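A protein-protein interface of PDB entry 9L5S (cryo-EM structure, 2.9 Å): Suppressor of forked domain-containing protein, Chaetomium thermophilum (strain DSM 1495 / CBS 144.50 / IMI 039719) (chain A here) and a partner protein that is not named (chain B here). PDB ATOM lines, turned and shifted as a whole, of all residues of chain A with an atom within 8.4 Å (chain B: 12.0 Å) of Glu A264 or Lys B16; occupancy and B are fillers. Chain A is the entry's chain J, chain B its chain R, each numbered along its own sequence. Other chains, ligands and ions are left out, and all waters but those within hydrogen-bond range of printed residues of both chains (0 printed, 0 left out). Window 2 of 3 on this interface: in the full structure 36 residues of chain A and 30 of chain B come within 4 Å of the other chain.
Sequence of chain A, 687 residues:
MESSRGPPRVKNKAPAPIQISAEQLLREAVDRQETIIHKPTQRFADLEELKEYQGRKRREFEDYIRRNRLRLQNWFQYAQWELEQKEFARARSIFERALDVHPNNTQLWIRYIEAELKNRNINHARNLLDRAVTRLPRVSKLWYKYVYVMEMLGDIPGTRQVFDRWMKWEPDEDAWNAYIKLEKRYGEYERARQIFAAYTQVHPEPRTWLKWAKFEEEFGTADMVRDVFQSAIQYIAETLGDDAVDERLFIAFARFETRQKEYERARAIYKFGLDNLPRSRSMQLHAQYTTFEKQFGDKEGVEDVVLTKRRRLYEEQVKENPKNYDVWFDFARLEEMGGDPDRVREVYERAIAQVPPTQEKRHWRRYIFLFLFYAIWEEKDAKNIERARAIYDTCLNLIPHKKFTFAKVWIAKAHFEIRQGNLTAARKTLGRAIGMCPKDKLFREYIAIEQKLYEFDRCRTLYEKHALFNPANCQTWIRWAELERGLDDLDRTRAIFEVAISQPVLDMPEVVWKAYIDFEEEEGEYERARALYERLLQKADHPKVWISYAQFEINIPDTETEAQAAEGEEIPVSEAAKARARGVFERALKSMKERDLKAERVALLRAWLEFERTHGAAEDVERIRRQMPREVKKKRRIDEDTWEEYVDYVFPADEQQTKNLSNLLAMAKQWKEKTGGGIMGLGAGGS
The backbone carbonyl oxygen (O) of Lys A261 sits close to the side-chain hydroxyl (OH) of Tyr B17 (3.4 Å).
The side-chain carboxylate of Glu A264 is in salt-bridge range of the side-chain amino group of Lys B16 (2.8 Å).
The backbone NH (N) of Lys B16 sits at hydrogen-bond distance from the side-chain carboxylate (OE2) of Glu A262, 2.8 Å away.
The side-chain carboxylate (OE2) of Glu A262 sits at hydrogen-bond distance from the backbone NH (N) of Tyr B17 (3.1 Å).
The side-chain carboxylate of Glu A257 is in salt-bridge range of the guanidinium group of Arg A265 (3.2 Å).
The backbone carbonyl oxygen (O) of Glu A257 sits at hydrogen-bond distance from the backbone NH (N) of Glu A262 (2.7 Å).
Among the printed residues, pairs that only touch across the chains: Gln A260 with Tyr B17 (3.6 Å), Lys A261 with Lys B16 (3.5 Å), Glu A262 with Pro B15 (3.5 Å), Tyr A263 with Lys B16 (3.7 Å), Glu A264 with Pro B13 (3.8 Å), Arg A265 with Leu B12 (3.3 Å), Arg A265 with Pro B13 (3.4 Å), Arg A265 with Pro B15 (3.3 Å), Ile A269 with Leu B8 (3.8 Å) and Ile A269 with Leu B12 (3.6 Å).
Of the printed residues of chain B, Lys A261 touches Lys B16 (3.5 Å) and Tyr B17 (3.1 Å).
Glu A262 touches just these residues of chain B: Pro B15, Lys B16 and Tyr B17.
Of chain B, only Lys B16 comes within 4 Å of Tyr A263.
Glu A264 touches two residues of chain B.
Of the printed residues of chain B, Arg A265 touches Leu B12 (3.3 Å), Pro B13 (3.4 Å) and Pro B15 (3.3 Å).
Ala A268 touches none of the printed residues of chain B.
Gly B7 touches none of the printed residues of chain A.
Of the printed residues of chain A, Leu B8 touches Ile A269.
Printed residues of chain A within 4 Å of Pro B13: Glu A264 and Arg A265.
Lys B16 touches just these residues of chain A: Lys A261, Glu A262, Tyr A263 and Glu A264.
Glu B22 touches none of the printed residues of chain A.
The nearest residue of chain B that does not touch Glu A264 is Lys B14 (4.5 Å).
The nearest residue of chain A that does not touch Lys B16 is Arg A265 (5.9 Å).
The nearest printed residue of chain A that does not touch Tyr B17 is Tyr A263 (5.0 Å).
Hydrophobic or aromatic side chains of chain A within 4 Å of the printed part of chain B: Ile A269.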
ATOM      1  N   ARG A 226      -7.096 -27.610  34.913  1.00  0.00           N
ATOM      2  CA  ARG A 226      -7.643 -28.705  34.116  1.00  0.00           C
ATOM      3  C   ARG A 226      -7.684 -30.001  34.917  1.00  0.00           C
ATOM      4  O   ARG A 226      -8.668 -30.748  34.851  1.00  0.00           O
ATOM      5  CB  ARG A 226      -6.812 -28.884  32.845  1.00  0.00           C
ATOM      6  CG  ARG A 226      -7.047 -27.810  31.794  1.00  0.00           C
ATOM      7  CD  ARG A 226      -6.009 -27.883  30.685  1.00  0.00           C
ATOM      8  NE  ARG A 226      -6.051 -26.708  29.823  1.00  0.00           N
ATOM      9  CZ  ARG A 226      -4.980 -26.069  29.373  1.00  0.00           C
ATOM     10  NH1 ARG A 226      -3.757 -26.468  29.682  1.00  0.00           N
ATOM     11  NH2 ARG A 226      -5.140 -25.004  28.593  1.00  0.00           N
ATOM     12  N   GLU A 257     -12.028 -22.060  29.884  1.00  0.00           N
ATOM     13  CA  GLU A 257     -11.454 -22.295  28.563  1.00  0.00           C
ATOM     14  C   GLU A 257     -11.627 -21.080  27.654  1.00  0.00           C
ATOM     15  O   GLU A 257     -10.725 -20.754  26.872  1.00  0.00           O
ATOM     16  CB  GLU A 257     -12.078 -23.542  27.936  1.00  0.00           C
ATOM     17  CG  GLU A 257     -11.671 -24.845  28.617  1.00  0.00           C
ATOM     18  CD  GLU A 257     -10.175 -25.093  28.572  1.00  0.00           C
ATOM     19  OE1 GLU A 257      -9.558 -24.834  27.522  1.00  0.00           O
ATOM     20  OE2 GLU A 257      -9.610 -25.540  29.591  1.00  0.00           O
ATOM     21  N   THR A 258     -12.782 -20.408  27.731  1.00  0.00           N
ATOM     22  CA  THR A 258     -12.993 -19.204  26.925  1.00  0.00           C
ATOM     23  C   THR A 258     -12.089 -18.061  27.372  1.00  0.00           C
ATOM     24  O   THR A 258     -11.556 -17.325  26.536  1.00  0.00           O
ATOM     25  CB  THR A 258     -14.455 -18.751  26.969  1.00  0.00           C
ATOM     26  OG1 THR A 258     -14.824 -18.431  28.316  1.00  0.00           O
ATOM     27  CG2 THR A 258     -15.383 -19.809  26.398  1.00  0.00           C
ATOM     28  N   GLN A 260      -9.258 -18.511  28.664  1.00  0.00           N
ATOM     29  CA  GLN A 260      -7.966 -18.931  28.144  1.00  0.00           C
ATOM     30  C   GLN A 260      -7.952 -18.961  26.620  1.00  0.00           C
ATOM     31  O   GLN A 260      -6.961 -19.405  26.029  1.00  0.00           O
ATOM     32  CB  GLN A 260      -7.581 -20.300  28.709  1.00  0.00           C
ATOM     33  CG  GLN A 260      -7.022 -20.248  30.123  1.00  0.00           C
ATOM     34  CD  GLN A 260      -5.683 -19.538  30.186  1.00  0.00           C
ATOM     35  OE1 GLN A 260      -5.486 -18.630  30.993  1.00  0.00           O
ATOM     36  NE2 GLN A 260      -4.756 -19.948  29.328  1.00  0.00           N
ATOM     37  N   LYS A 261      -9.044 -18.514  25.986  1.00  0.00           N
ATOM     38  CA  LYS A 261      -9.171 -18.379  24.528  1.00  0.00           C
ATOM     39  C   LYS A 261      -8.995 -19.715  23.806  1.00  0.00           C
ATOM     40  O   LYS A 261      -8.506 -19.772  22.676  1.00  0.00           O
ATOM     41  CB  LYS A 261      -8.209 -17.319  23.981  1.00  0.00           C
ATOM     42  CG  LYS A 261      -8.647 -15.893  24.298  1.00  0.00           C
ATOM     43  CD  LYS A 261      -7.498 -14.904  24.193  1.00  0.00           C
ATOM     44  CE  LYS A 261      -7.027 -14.742  22.758  1.00  0.00           C
ATOM     45  NZ  LYS A 261      -5.951 -13.720  22.648  1.00  0.00           N
ATOM     46  N   GLU A 262      -9.418 -20.796  24.454  1.00  0.00           N
ATOM     47  CA  GLU A 262      -9.438 -22.138  23.870  1.00  0.00           C
ATOM     48  C   GLU A 262     -10.877 -22.443  23.461  1.00  0.00           C
ATOM     49  O   GLU A 262     -11.641 -23.054  24.210  1.00  0.00           O
ATOM     50  CB  GLU A 262      -8.900 -23.169  24.848  1.00  0.00           C
ATOM     51  CG  GLU A 262      -7.412 -23.064  25.118  1.00  0.00           C
ATOM     52  CD  GLU A 262      -6.582 -23.714  24.024  1.00  0.00           C
ATOM     53  OE1 GLU A 262      -7.146 -24.493  23.228  1.00  0.00           O
ATOM     54  OE2 GLU A 262      -5.365 -23.446  23.958  1.00  0.00           O
ATOM     55  N   TYR A 263     -11.235 -22.017  22.251  1.00  0.00           N
ATOM     56  CA  TYR A 263     -12.635 -22.001  21.843  1.00  0.00           C
ATOM     57  C   TYR A 263     -13.146 -23.391  21.484  1.00  0.00           C
ATOM     58  O   TYR A 263     -14.284 -23.738  21.820  1.00  0.00           O
ATOM     59  CB  TYR A 263     -12.814 -21.034  20.674  1.00  0.00           C
ATOM     60  CG  TYR A 263     -12.525 -19.605  21.065  1.00  0.00           C
ATOM     61  CD1 TYR A 263     -11.232 -19.093  20.995  1.00  0.00           C
ATOM     62  CD2 TYR A 263     -13.532 -18.777  21.537  1.00  0.00           C
ATOM     63  CE1 TYR A 263     -10.956 -17.796  21.364  1.00  0.00           C
ATOM     64  CE2 TYR A 263     -13.264 -17.478  21.909  1.00  0.00           C
ATOM     65  CZ  TYR A 263     -11.975 -16.992  21.819  1.00  0.00           C
ATOM     66  OH  TYR A 263     -11.692 -15.698  22.185  1.00  0.00           O
ATOM     67  N   GLU A 264     -12.329 -24.197  20.800  1.00  0.00           N
ATOM     68  CA  GLU A 264     -12.739 -25.562  20.482  1.00  0.00           C
ATOM     69  C   GLU A 264     -12.805 -26.435  21.732  1.00  0.00           C
ATOM     70  O   GLU A 264     -13.662 -27.322  21.819  1.00  0.00           O
ATOM     71  CB  GLU A 264     -11.803 -26.165  19.428  1.00  0.00           C
ATOM     72  CG  GLU A 264     -10.355 -26.371  19.867  1.00  0.00           C
ATOM     73  CD  GLU A 264      -9.488 -25.144  19.642  1.00  0.00           C
ATOM     74  OE1 GLU A 264     -10.040 -24.067  19.332  1.00  0.00           O
ATOM     75  OE2 GLU A 264      -8.252 -25.254  19.790  1.00  0.00           O
ATOM     76  N   ARG A 265     -11.937 -26.175  22.718  1.00  0.00           N
ATOM     77  CA  ARG A 265     -12.008 -26.880  23.993  1.00  0.00           C
ATOM     78  C   ARG A 265     -13.322 -26.584  24.707  1.00  0.00           C
ATOM     79  O   ARG A 265     -14.008 -27.498  25.182  1.00  0.00           O
ATOM     80  CB  ARG A 265     -10.828 -26.478  24.880  1.00  0.00           C
ATOM     81  CG  ARG A 265      -9.437 -26.689  24.289  1.00  0.00           C
ATOM     82  CD  ARG A 265      -8.849 -28.042  24.653  1.00  0.00           C
ATOM     83  NE  ARG A 265      -8.944 -28.316  26.084  1.00  0.00           N
ATOM     84  CZ  ARG A 265      -8.139 -27.831  27.018  1.00  0.00           C
ATOM     85  NH1 ARG A 265      -7.137 -27.021  26.719  1.00  0.00           N
ATOM     86  NH2 ARG A 265      -8.346 -28.166  28.288  1.00  0.00           N
ATOM     87  N   ALA A 266     -13.690 -25.302  24.778  1.00  0.00           N
ATOM     88  CA  ALA A 266     -14.934 -24.915  25.435  1.00  0.00           C
ATOM     89  C   ALA A 266     -16.146 -25.427  24.670  1.00  0.00           C
ATOM     90  O   ALA A 266     -17.154 -25.801  25.280  1.00  0.00           O
ATOM     91  CB  ALA A 266     -14.994 -23.397  25.588  1.00  0.00           C
ATOM     92  N   ARG A 267     -16.064 -25.455  23.337  1.00  0.00           N
ATOM     93  CA  ARG A 267     -17.143 -26.025  22.537  1.00  0.00           C
ATOM     94  C   ARG A 267     -17.301 -27.517  22.807  1.00  0.00           C
ATOM     95  O   ARG A 267     -18.428 -28.025  22.877  1.00  0.00           O
ATOM     96  CB  ARG A 267     -16.882 -25.767  21.054  1.00  0.00           C
ATOM     97  CG  ARG A 267     -17.847 -24.782  20.420  1.00  0.00           C
ATOM     98  CD  ARG A 267     -17.888 -24.940  18.908  1.00  0.00           C
ATOM     99  NE  ARG A 267     -16.754 -24.296  18.253  1.00  0.00           N
ATOM    100  CZ  ARG A 267     -16.662 -22.994  18.014  1.00  0.00           C
ATOM    101  NH1 ARG A 267     -17.628 -22.157  18.357  1.00  0.00           N
ATOM    102  NH2 ARG A 267     -15.577 -22.522  17.409  1.00  0.00           N
ATOM    103  N   ALA A 268     -16.180 -28.232  22.963  1.00  0.00           N
ATOM    104  CA  ALA A 268     -16.233 -29.648  23.310  1.00  0.00           C
ATOM    105  C   ALA A 268     -16.863 -29.864  24.680  1.00  0.00           C
ATOM    106  O   ALA A 268     -17.684 -30.773  24.857  1.00  0.00           O
ATOM    107  CB  ALA A 268     -14.828 -30.249  23.267  1.00  0.00           C
ATOM    108  N   ILE A 269     -16.495 -29.026  25.658  1.00  0.00           N
ATOM    109  CA  ILE A 269     -17.103 -29.099  26.989  1.00  0.00           C
ATOM    110  C   ILE A 269     -18.602 -28.850  26.916  1.00  0.00           C
ATOM    111  O   ILE A 269     -19.395 -29.574  27.529  1.00  0.00           O
ATOM    112  CB  ILE A 269     -16.410 -28.118  27.953  1.00  0.00           C
ATOM    113  CG1 ILE A 269     -14.930 -28.453  28.069  1.00  0.00           C
ATOM    114  CG2 ILE A 269     -17.068 -28.138  29.324  1.00  0.00           C
ATOM    115  CD1 ILE A 269     -14.699 -29.830  28.614  1.00  0.00           C
ATOM    116  N   TYR A 270     -19.012 -27.833  26.155  1.00  0.00           N
ATOM    117  CA  TYR A 270     -20.427 -27.495  26.054  1.00  0.00           C
ATOM    118  C   TYR A 270     -21.227 -28.612  25.392  1.00  0.00           C
ATOM    119  O   TYR A 270     -22.303 -28.981  25.879  1.00  0.00           O
ATOM    120  CB  TYR A 270     -20.590 -26.190  25.282  1.00  0.00           C
ATOM    121  CG  TYR A 270     -20.508 -24.943  26.134  1.00  0.00           C
ATOM    122  CD1 TYR A 270     -21.331 -24.777  27.238  1.00  0.00           C
ATOM    123  CD2 TYR A 270     -19.624 -23.920  25.818  1.00  0.00           C
ATOM    124  CE1 TYR A 270     -21.261 -23.637  28.018  1.00  0.00           C
ATOM    125  CE2 TYR A 270     -19.547 -22.775  26.587  1.00  0.00           C
ATOM    126  CZ  TYR A 270     -20.368 -22.638  27.687  1.00  0.00           C
ATOM    127  OH  TYR A 270     -20.298 -21.500  28.458  1.00  0.00           O
ATOM    128  N   LYS A 271     -20.709 -29.187  24.301  1.00  0.00           N
ATOM    129  CA  LYS A 271     -21.462 -30.239  23.621  1.00  0.00           C
ATOM    130  C   LYS A 271     -21.484 -31.532  24.432  1.00  0.00           C
ATOM    131  O   LYS A 271     -22.492 -32.248  24.418  1.00  0.00           O
ATOM    132  CB  LYS A 271     -20.912 -30.471  22.206  1.00  0.00           C
ATOM    133  CG  LYS A 271     -19.476 -30.977  22.094  1.00  0.00           C
ATOM    134  CD  LYS A 271     -19.391 -32.487  21.908  1.00  0.00           C
ATOM    135  CE  LYS A 271     -17.950 -32.936  21.745  1.00  0.00           C
ATOM    136  NZ  LYS A 271     -17.845 -34.414  21.610  1.00  0.00           N
ATOM    137  N   PHE A 292     -22.469 -18.161  24.554  1.00  0.00           N
ATOM    138  CA  PHE A 292     -21.115 -18.304  24.024  1.00  0.00           C
ATOM    139  C   PHE A 292     -21.110 -18.267  22.499  1.00  0.00           C
ATOM    140  O   PHE A 292     -20.237 -17.632  21.890  1.00  0.00           O
ATOM    141  CB  PHE A 292     -20.490 -19.601  24.539  1.00  0.00           C
ATOM    142  CG  PHE A 292     -19.277 -20.044  23.769  1.00  0.00           C
ATOM    143  CD1 PHE A 292     -18.118 -19.282  23.774  1.00  0.00           C
ATOM    144  CD2 PHE A 292     -19.294 -21.226  23.046  1.00  0.00           C
ATOM    145  CE1 PHE A 292     -17.000 -19.690  23.069  1.00  0.00           C
ATOM    146  CE2 PHE A 292     -18.180 -21.640  22.338  1.00  0.00           C
ATOM    147  CZ  PHE A 292     -17.032 -20.869  22.350  1.00  0.00           C
ATOM    148  N   GLY B   7     -14.674 -40.498  28.430  1.00  0.00           N
ATOM    149  CA  GLY B   7     -15.245 -39.973  27.201  1.00  0.00           C
ATOM    150  C   GLY B   7     -14.923 -38.508  26.980  1.00  0.00           C
ATOM    151  O   GLY B   7     -14.601 -38.097  25.861  1.00  0.00           O
ATOM    152  N   LEU B   8     -14.984 -37.702  28.042  1.00  0.00           N
ATOM    153  CA  LEU B   8     -14.643 -36.293  27.887  1.00  0.00           C
ATOM    154  C   LEU B   8     -13.138 -36.106  27.723  1.00  0.00           C
ATOM    155  O   LEU B   8     -12.702 -35.239  26.960  1.00  0.00           O
ATOM    156  CB  LEU B   8     -15.188 -35.478  29.061  1.00  0.00           C
ATOM    157  CG  LEU B   8     -14.936 -33.972  28.949  1.00  0.00           C
ATOM    158  CD1 LEU B   8     -15.638 -33.441  27.732  1.00  0.00           C
ATOM    159  CD2 LEU B   8     -15.440 -33.233  30.159  1.00  0.00           C
ATOM    160  N   ALA B   9     -12.328 -36.936  28.392  1.00  0.00           N
ATOM    161  CA  ALA B   9     -10.881 -36.877  28.198  1.00  0.00           C
ATOM    162  C   ALA B   9     -10.493 -37.223  26.768  1.00  0.00           C
ATOM    163  O   ALA B   9      -9.517 -36.679  26.239  1.00  0.00           O
ATOM    164  CB  ALA B   9     -10.182 -37.814  29.182  1.00  0.00           C
ATOM    165  N   ALA B  10     -11.240 -38.125  26.128  1.00  0.00           N
ATOM    166  CA  ALA B  10     -11.044 -38.357  24.702  1.00  0.00           C
ATOM    167  C   ALA B  10     -11.686 -37.262  23.855  1.00  0.00           C
ATOM    168  O   ALA B  10     -11.328 -37.099  22.684  1.00  0.00           O
ATOM    169  CB  ALA B  10     -11.602 -39.725  24.311  1.00  0.00           C
ATOM    170  N   ALA B  11     -12.631 -36.506  24.424  1.00  0.00           N
ATOM    171  CA  ALA B  11     -13.361 -35.522  23.631  1.00  0.00           C
ATOM    172  C   ALA B  11     -12.534 -34.266  23.369  1.00  0.00           C
ATOM    173  O   ALA B  11     -12.674 -33.644  22.309  1.00  0.00           O
ATOM    174  CB  ALA B  11     -14.676 -35.159  24.320  1.00  0.00           C
ATOM    175  N   LEU B  12     -11.684 -33.865  24.315  1.00  0.00           N
ATOM    176  CA  LEU B  12     -10.972 -32.603  24.157  1.00  0.00           C
ATOM    177  C   LEU B  12      -9.848 -32.750  23.133  1.00  0.00           C
ATOM    178  O   LEU B  12      -9.258 -33.828  23.005  1.00  0.00           O
ATOM    179  CB  LEU B  12     -10.372 -32.103  25.475  1.00  0.00           C
ATOM    180  CG  LEU B  12     -11.216 -31.326  26.493  1.00  0.00           C
ATOM    181  CD1 LEU B  12     -11.716 -30.007  25.935  1.00  0.00           C
ATOM    182  CD2 LEU B  12     -12.337 -32.112  27.065  1.00  0.00           C
ATOM    183  N   PRO B  13      -9.534 -31.690  22.388  1.00  0.00           N
ATOM    184  CA  PRO B  13      -8.321 -31.703  21.564  1.00  0.00           C
ATOM    185  C   PRO B  13      -7.120 -31.153  22.317  1.00  0.00           C
ATOM    186  O   PRO B  13      -7.228 -30.774  23.489  1.00  0.00           O
ATOM    187  CB  PRO B  13      -8.692 -30.814  20.368  1.00  0.00           C
ATOM    188  CG  PRO B  13      -9.928 -30.043  20.787  1.00  0.00           C
ATOM    189  CD  PRO B  13     -10.343 -30.483  22.161  1.00  0.00           C
ATOM    190  N   LYS B  14      -5.973 -31.113  21.649  1.00  0.00           N
ATOM    191  CA  LYS B  14      -4.779 -30.522  22.226  1.00  0.00           C
ATOM    192  C   LYS B  14      -4.964 -29.005  22.312  1.00  0.00           C
ATOM    193  O   LYS B  14      -5.467 -28.385  21.371  1.00  0.00           O
ATOM    194  CB  LYS B  14      -3.573 -30.861  21.348  1.00  0.00           C
ATOM    195  CG  LYS B  14      -2.204 -30.386  21.812  1.00  0.00           C
ATOM    196  CD  LYS B  14      -1.752 -31.104  23.078  1.00  0.00           C
ATOM    197  CE  LYS B  14      -0.392 -30.609  23.537  1.00  0.00           C
ATOM    198  NZ  LYS B  14       0.677 -30.967  22.564  1.00  0.00           N
ATOM    199  N   PRO B  15      -4.602 -28.384  23.441  1.00  0.00           N
ATOM    200  CA  PRO B  15      -4.711 -26.922  23.536  1.00  0.00           C
ATOM    201  C   PRO B  15      -3.768 -26.219  22.572  1.00  0.00           C
ATOM    202  O   PRO B  15      -2.619 -26.625  22.383  1.00  0.00           O
ATOM    203  CB  PRO B  15      -4.345 -26.613  24.993  1.00  0.00           C
ATOM    204  CG  PRO B  15      -3.813 -27.852  25.576  1.00  0.00           C
ATOM    205  CD  PRO B  15      -4.115 -29.005  24.684  1.00  0.00           C
ATOM    206  N   LYS B  16      -4.274 -25.143  21.965  1.00  0.00           N
ATOM    207  CA  LYS B  16      -3.578 -24.438  20.896  1.00  0.00           C
ATOM    208  C   LYS B  16      -2.542 -23.432  21.389  1.00  0.00           C
ATOM    209  O   LYS B  16      -1.675 -23.038  20.602  1.00  0.00           O
ATOM    210  CB  LYS B  16      -4.604 -23.754  19.989  1.00  0.00           C
ATOM    211  CG  LYS B  16      -5.269 -22.526  20.599  1.00  0.00           C
ATOM    212  CD  LYS B  16      -5.861 -21.632  19.524  1.00  0.00           C
ATOM    213  CE  LYS B  16      -7.169 -22.201  19.008  1.00  0.00           C
ATOM    214  NZ  LYS B  16      -8.269 -22.070  20.004  1.00  0.00           N
ATOM    215  N   TYR B  17      -2.589 -23.018  22.652  1.00  0.00           N
ATOM    216  CA  TYR B  17      -1.500 -22.251  23.257  1.00  0.00           C
ATOM    217  C   TYR B  17      -0.735 -23.195  24.176  1.00  0.00           C
ATOM    218  O   TYR B  17      -1.249 -23.626  25.212  1.00  0.00           O
ATOM    219  CB  TYR B  17      -1.983 -21.012  24.014  1.00  0.00           C
ATOM    220  CG  TYR B  17      -3.043 -20.177  23.325  1.00  0.00           C
ATOM    221  CD1 TYR B  17      -2.686 -19.073  22.553  1.00  0.00           C
ATOM    222  CD2 TYR B  17      -4.395 -20.460  23.481  1.00  0.00           C
ATOM    223  CE1 TYR B  17      -3.648 -18.294  21.927  1.00  0.00           C
ATOM    224  CE2 TYR B  17      -5.364 -19.687  22.862  1.00  0.00           C
ATOM    225  CZ  TYR B  17      -4.984 -18.606  22.087  1.00  0.00           C
ATOM    226  OH  TYR B  17      -5.946 -17.832  21.473  1.00  0.00           O
ATOM    227  N   SER B  18       0.489 -23.524  23.778  1.00  0.00           N
ATOM    228  CA  SER B  18       1.338 -24.389  24.582  1.00  0.00           C
ATOM    229  C   SER B  18       1.826 -23.647  25.820  1.00  0.00           C
ATOM    230  O   SER B  18       2.279 -22.499  25.733  1.00  0.00           O
ATOM    231  CB  SER B  18       2.521 -24.879  23.750  1.00  0.00           C
ATOM    232  OG  SER B  18       3.367 -23.802  23.393  1.00  0.00           O
ATOM    233  N   SER B  19       1.733 -24.301  26.974  1.00  0.00           N
ATOM    234  CA  SER B  19       2.087 -23.705  28.257  1.00  0.00           C
ATOM    235  C   SER B  19       3.080 -24.577  29.016  1.00  0.00           C
ATOM    236  O   SER B  19       2.940 -24.804  30.219  1.00  0.00           O
ATOM    237  CB  SER B  19       0.841 -23.455  29.104  1.00  0.00           C
ATOM    238  OG  SER B  19      -0.050 -22.563  28.457  1.00  0.00           O
ATOM    239  N   GLU B  20       4.098 -25.083  28.318  1.00  0.00           N
ATOM    240  CA  GLU B  20       5.151 -25.851  28.970  1.00  0.00           C
ATOM    241  C   GLU B  20       6.150 -24.970  29.709  1.00  0.00           C
ATOM    242  O   GLU B  20       6.945 -25.490  30.501  1.00  0.00           O
ATOM    243  CB  GLU B  20       5.886 -26.719  27.944  1.00  0.00           C
ATOM    244  CG  GLU B  20       6.910 -25.976  27.099  1.00  0.00           C
ATOM    245  CD  GLU B  20       6.325 -25.433  25.807  1.00  0.00           C
ATOM    246  OE1 GLU B  20       5.095 -25.238  25.742  1.00  0.00           O
ATOM    247  OE2 GLU B  20       7.099 -25.208  24.852  1.00  0.00           O
ATOM    248  N   HIS B  21       6.132 -23.659  29.469  1.00  0.00           N
ATOM    249  CA  HIS B  21       6.973 -22.707  30.179  1.00  0.00           C
ATOM    250  C   HIS B  21       6.203 -21.956  31.259  1.00  0.00           C
ATOM    251  O   HIS B  21       6.630 -20.875  31.680  1.00  0.00           O
ATOM    252  CB  HIS B  21       7.590 -21.711  29.196  1.00  0.00           C
ATOM    253  CG  HIS B  21       8.492 -22.340  28.180  1.00  0.00           C
ATOM    254  ND1 HIS B  21       8.061 -22.692  26.921  1.00  0.00           N
ATOM    255  CD2 HIS B  21       9.803 -22.677  28.238  1.00  0.00           C
ATOM    256  CE1 HIS B  21       9.066 -23.219  26.245  1.00  0.00           C
ATOM    257  NE2 HIS B  21      10.134 -23.222  27.021  1.00  0.00           N
ATOM    258  N   GLU B  22       5.082 -22.508  31.717  1.00  0.00           N
ATOM    259  CA  GLU B  22       4.157 -21.785  32.585  1.00  0.00           C
ATOM    260  C   GLU B  22       4.646 -21.879  34.025  1.00  0.00           C
ATOM    261  O   GLU B  22       4.385 -22.862  34.724  1.00  0.00           O
ATOM    262  CB  GLU B  22       2.742 -22.335  32.435  1.00  0.00           C
ATOM    263  CG  GLU B  22       1.698 -21.625  33.285  1.00  0.00           C
ATOM    264  CD  GLU B  22       1.552 -20.156  32.937  1.00  0.00           C
ATOM    265  OE1 GLU B  22       1.647 -19.811  31.740  1.00  0.00           O
ATOM    266  OE2 GLU B  22       1.342 -19.345  33.863  1.00  0.00           O
